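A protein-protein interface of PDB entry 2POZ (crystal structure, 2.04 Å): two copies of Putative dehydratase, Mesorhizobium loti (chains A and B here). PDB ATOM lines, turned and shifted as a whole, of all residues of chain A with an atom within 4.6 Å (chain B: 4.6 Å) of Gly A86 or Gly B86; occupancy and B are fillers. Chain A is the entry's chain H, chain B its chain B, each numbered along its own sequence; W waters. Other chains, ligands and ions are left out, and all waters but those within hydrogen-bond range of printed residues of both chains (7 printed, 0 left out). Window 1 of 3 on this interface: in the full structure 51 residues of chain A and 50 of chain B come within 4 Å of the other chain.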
ATOM      1  N   ASN A  84      21.868  13.733 -21.186  1.00  0.00           N
ATOM      2  CA  ASN A  84      22.743  14.458 -20.269  1.00  0.00           C
ATOM      3  C   ASN A  84      23.521  13.399 -19.495  1.00  0.00           C
ATOM      4  O   ASN A  84      23.990  13.640 -18.381  1.00  0.00           O
ATOM      5  CB  ASN A  84      21.973  15.359 -19.300  1.00  0.00           C
ATOM      6  CG  ASN A  84      22.894  16.339 -18.569  1.00  0.00           C
ATOM      7  OD1 ASN A  84      23.780  16.943 -19.181  1.00  0.00           O
ATOM      8  ND2 ASN A  84      22.695  16.493 -17.264  1.00  0.00           N
ATOM      9  N   GLY A  85      23.666  12.228 -20.118  1.00  0.00           N
ATOM     10  CA  GLY A  85      24.370  11.107 -19.505  1.00  0.00           C
ATOM     11  C   GLY A  85      25.855  11.278 -19.238  1.00  0.00           C
ATOM     12  O   GLY A  85      26.522  12.113 -19.858  1.00  0.00           O
ATOM     13  N   GLY A  86      26.375  10.459 -18.326  1.00  0.00           N
ATOM     14  CA  GLY A  86      27.779  10.535 -17.960  1.00  0.00           C
ATOM     15  C   GLY A  86      28.675   9.402 -18.444  1.00  0.00           C
ATOM     16  O   GLY A  86      28.324   8.657 -19.358  1.00  0.00           O
ATOM     17  N   ALA A  87      29.834   9.273 -17.804  1.00  0.00           N
ATOM     18  CA  ALA A  87      30.839   8.267 -18.155  1.00  0.00           C
ATOM     19  C   ALA A  87      30.393   6.802 -18.154  1.00  0.00           C
ATOM     20  O   ALA A  87      30.808   6.036 -19.018  1.00  0.00           O
ATOM     21  CB  ALA A  87      32.062   8.423 -17.248  1.00  0.00           C
ATOM     22  N   ILE A  88      29.566   6.401 -17.196  1.00  0.00           N
ATOM     23  CA  ILE A  88      29.149   5.004 -17.145  1.00  0.00           C
ATOM     24  C   ILE A  88      28.205   4.604 -18.290  1.00  0.00           C
ATOM     25  O   ILE A  88      28.468   3.639 -19.005  1.00  0.00           O
ATOM     26  CB  ILE A  88      28.513   4.675 -15.783  1.00  0.00           C
ATOM     27  CG1 ILE A  88      29.479   5.062 -14.655  1.00  0.00           C
ATOM     28  CG2 ILE A  88      28.189   3.188 -15.702  1.00  0.00           C
ATOM     29  CD1 ILE A  88      30.874   4.415 -14.764  1.00  0.00           C
ATOM     30  N   ILE A  89      27.121   5.345 -18.478  1.00  0.00           N
ATOM     31  CA  ILE A  89      26.184   5.030 -19.552  1.00  0.00           C
ATOM     32  C   ILE A  89      26.858   5.089 -20.930  1.00  0.00           C
ATOM     33  O   ILE A  89      26.674   4.198 -21.764  1.00  0.00           O
ATOM     34  CB  ILE A  89      24.969   5.989 -19.531  1.00  0.00           C
ATOM     35  CG1 ILE A  89      24.015   5.662 -20.685  1.00  0.00           C
ATOM     36  CG2 ILE A  89      25.431   7.421 -19.646  1.00  0.00           C
ATOM     37  CD1 ILE A  89      23.330   4.332 -20.559  1.00  0.00           C
ATOM     38  N   PHE A  90      27.655   6.124 -21.169  1.00  0.00           N
ATOM     39  CA  PHE A  90      28.319   6.244 -22.457  1.00  0.00           C
ATOM     40  C   PHE A  90      29.535   5.333 -22.642  1.00  0.00           C
ATOM     41  O   PHE A  90      29.956   5.082 -23.766  1.00  0.00           O
ATOM     42  CB  PHE A  90      28.659   7.711 -22.735  1.00  0.00           C
ATOM     43  CG  PHE A  90      27.452   8.530 -23.097  1.00  0.00           C
ATOM     44  CD1 PHE A  90      27.024   9.579 -22.289  1.00  0.00           C
ATOM     45  CD2 PHE A  90      26.698   8.203 -24.226  1.00  0.00           C
ATOM     46  CE1 PHE A  90      25.856  10.294 -22.597  1.00  0.00           C
ATOM     47  CE2 PHE A  90      25.532   8.906 -24.540  1.00  0.00           C
ATOM     48  CZ  PHE A  90      25.111   9.952 -23.723  1.00  0.00           C
ATOM     49  N   TYR A 260      31.626  13.899 -22.624  1.00  0.00           N
ATOM     50  CA  TYR A 260      31.023  12.827 -23.413  1.00  0.00           C
ATOM     51  C   TYR A 260      30.050  13.223 -24.516  1.00  0.00           C
ATOM     52  O   TYR A 260      29.145  14.028 -24.304  1.00  0.00           O
ATOM     53  CB  TYR A 260      30.353  11.842 -22.452  1.00  0.00           C
ATOM     54  CG  TYR A 260      31.176  11.650 -21.199  1.00  0.00           C
ATOM     55  CD1 TYR A 260      30.888  12.362 -20.032  1.00  0.00           C
ATOM     56  CD2 TYR A 260      32.298  10.824 -21.207  1.00  0.00           C
ATOM     57  CE1 TYR A 260      31.705  12.254 -18.898  1.00  0.00           C
ATOM     58  CE2 TYR A 260      33.123  10.710 -20.083  1.00  0.00           C
ATOM     59  CZ  TYR A 260      32.821  11.425 -18.933  1.00  0.00           C
ATOM     60  OH  TYR A 260      33.634  11.295 -17.829  1.00  0.00           O
ATOM     61  N   ASN B  84      32.441  16.065 -13.323  1.00  0.00           N
ATOM     62  CA  ASN B  84      31.563  16.213 -14.480  1.00  0.00           C
ATOM     63  C   ASN B  84      30.835  14.878 -14.627  1.00  0.00           C
ATOM     64  O   ASN B  84      30.460  14.465 -15.726  1.00  0.00           O
ATOM     65  CB  ASN B  84      32.333  16.540 -15.763  1.00  0.00           C
ATOM     66  CG  ASN B  84      31.405  16.957 -16.898  1.00  0.00           C
ATOM     67  OD1 ASN B  84      30.469  17.730 -16.688  1.00  0.00           O
ATOM     68  ND2 ASN B  84      31.657  16.450 -18.100  1.00  0.00           N
ATOM     69  N   GLY B  85      30.638  14.222 -13.488  1.00  0.00           N
ATOM     70  CA  GLY B  85      29.982  12.927 -13.446  1.00  0.00           C
ATOM     71  C   GLY B  85      28.497  12.920 -13.756  1.00  0.00           C
ATOM     72  O   GLY B  85      27.833  13.962 -13.755  1.00  0.00           O
ATOM     73  N   GLY B  86      27.973  11.721 -13.996  1.00  0.00           N
ATOM     74  CA  GLY B  86      26.571  11.570 -14.328  1.00  0.00           C
ATOM     75  C   GLY B  86      25.719  10.821 -13.322  1.00  0.00           C
ATOM     76  O   GLY B  86      26.087  10.640 -12.156  1.00  0.00           O
ATOM     77  N   ALA B  87      24.568  10.362 -13.806  1.00  0.00           N
ATOM     78  CA  ALA B  87      23.587   9.668 -12.994  1.00  0.00           C
ATOM     79  C   ALA B  87      24.064   8.439 -12.228  1.00  0.00           C
ATOM     80  O   ALA B  87      23.656   8.228 -11.082  1.00  0.00           O
ATOM     81  CB  ALA B  87      22.380   9.305 -13.861  1.00  0.00           C
ATOM     82  N   ILE B  88      24.914   7.622 -12.839  1.00  0.00           N
ATOM     83  CA  ILE B  88      25.360   6.420 -12.153  1.00  0.00           C
ATOM     84  C   ILE B  88      26.289   6.717 -10.977  1.00  0.00           C
ATOM     85  O   ILE B  88      26.030   6.281  -9.858  1.00  0.00           O
ATOM     86  CB  ILE B  88      26.045   5.424 -13.124  1.00  0.00           C
ATOM     87  CG1 ILE B  88      25.101   5.075 -14.278  1.00  0.00           C
ATOM     88  CG2 ILE B  88      26.409   4.139 -12.371  1.00  0.00           C
ATOM     89  CD1 ILE B  88      23.804   4.413 -13.835  1.00  0.00           C
ATOM     90  N   ILE B  89      27.362   7.458 -11.222  1.00  0.00           N
ATOM     91  CA  ILE B  89      28.282   7.790 -10.139  1.00  0.00           C
ATOM     92  C   ILE B  89      27.559   8.520  -9.004  1.00  0.00           C
ATOM     93  O   ILE B  89      27.719   8.164  -7.836  1.00  0.00           O
ATOM     94  CB  ILE B  89      29.480   8.654 -10.644  1.00  0.00           C
ATOM     95  CG1 ILE B  89      30.382   9.048  -9.470  1.00  0.00           C
ATOM     96  CG2 ILE B  89      28.980   9.902 -11.342  1.00  0.00           C
ATOM     97  CD1 ILE B  89      31.064   7.877  -8.782  1.00  0.00           C
ATOM     98  N   PHE B  90      26.743   9.519  -9.334  1.00  0.00           N
ATOM     99  CA  PHE B  90      26.041  10.253  -8.287  1.00  0.00           C
ATOM    100  C   PHE B  90      24.852   9.553  -7.650  1.00  0.00           C
ATOM    101  O   PHE B  90      24.433   9.933  -6.563  1.00  0.00           O
ATOM    102  CB  PHE B  90      25.670  11.658  -8.773  1.00  0.00           C
ATOM    103  CG  PHE B  90      26.865  12.561  -8.897  1.00  0.00           C
ATOM    104  CD1 PHE B  90      27.301  13.004 -10.136  1.00  0.00           C
ATOM    105  CD2 PHE B  90      27.613  12.887  -7.768  1.00  0.00           C
ATOM    106  CE1 PHE B  90      28.478  13.760 -10.254  1.00  0.00           C
ATOM    107  CE2 PHE B  90      28.787  13.640  -7.870  1.00  0.00           C
ATOM    108  CZ  PHE B  90      29.221  14.076  -9.116  1.00  0.00           C
ATOM    109  N   TYR B 260      22.672  16.825 -12.239  1.00  0.00           N
ATOM    110  CA  TYR B 260      23.292  16.352 -11.007  1.00  0.00           C
ATOM    111  C   TYR B 260      24.257  17.282 -10.264  1.00  0.00           C
ATOM    112  O   TYR B 260      25.133  17.890 -10.870  1.00  0.00           O
ATOM    113  CB  TYR B 260      23.974  15.014 -11.309  1.00  0.00           C
ATOM    114  CG  TYR B 260      23.157  14.157 -12.268  1.00  0.00           C
ATOM    115  CD1 TYR B 260      23.420  14.161 -13.643  1.00  0.00           C
ATOM    116  CD2 TYR B 260      22.073  13.412 -11.811  1.00  0.00           C
ATOM    117  CE1 TYR B 260      22.614  13.441 -14.540  1.00  0.00           C
ATOM    118  CE2 TYR B 260      21.255  12.690 -12.697  1.00  0.00           C
ATOM    119  CZ  TYR B 260      21.532  12.709 -14.056  1.00  0.00           C
ATOM    120  OH  TYR B 260      20.729  12.001 -14.925  1.00  0.00           O
HETATM  121  O   HOH W   1      32.911  12.159 -15.330  1.00  0.00           O
HETATM  122  O   HOH W   2      21.486  11.450 -17.403  1.00  0.00           O
HETATM  123  O   HOH W   3      24.201  17.705 -14.612  1.00  0.00           O
HETATM  124  O   HOH W   4      30.477   9.856 -14.659  1.00  0.00           O
HETATM  125  O   HOH W   5      24.119  11.365 -16.400  1.00  0.00           O
HETATM  126  O   HOH W   6      30.018  15.755 -20.991  1.00  0.00           O
HETATM  127  O   HOH W   7      25.906  13.776 -16.545  1.00  0.00           O
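Water W7 bridges the backbone carbonyl oxygen (O) of Asn A84 (2.7 Å) and the backbone carbonyl oxygen (O) of Gly B85 (3.4 Å).
Water W1 lies within hydrogen-bond range of OH of Tyr A260 (2.7 Å) and O of Asn B84 (3.4 Å).
Water W5 lies within hydrogen-bond range of N of Ala B87 (2.8 Å), O of Asn A84 (3.0 Å) and N of Gly A86 (3.1 Å).
Water W6 lies within hydrogen-bond range of N of Tyr A260 (2.9 Å) and ND2 of Asn B84 (3.4 Å).
Water W3 bridges the backbone NH of Tyr B260 (3.0 Å) and the side-chain amide nitrogen of Asn A84 (3.3 Å).
Water W4 lies within hydrogen-bond range of N of Gly B86 and N of Ala A87.
Gly B86 touches Gly A86.
Ile B88 touches Ile A88.
Of the 8 printed residues of chain A, 2 touch a printed residue of chain B.
Hydrophobic or aromatic side chains of chain A within 4 Å of the printed part of chain B: Ile A88.
Among the printed residues, no Asp or Glu carboxylate lies within 4 Å of a Lys or Arg side-chain nitrogen of the other chain.
Of chain B, only Gly B86 comes within 4 Å of Gly A86.
Gly B86 touches just one residue of chain A: Gly A86 (3.97 Å).
Printed residues of chain B within 4 Å of Ile A88: Ile B88 (3.7 Å).
Of the printed residues of chain A, Ile B88 touches Ile A88 (3.7 Å).
Asn A84 touches none of the printed residues of chain B.
The nearest printed residue of chain A that does not touch Gly B86 is Ala A87 (4.9 Å).
The nearest printed residue of chain A that does not touch Ile B88 is Ile A89 (4.7 Å).
Gly B86 touches its own counterpart, Gly A86.
Ile B88 touches its own counterpart, Ile A88.
Positions printed for both chains: 84, 85, 86, 87, 88, 89, 90 and 260.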
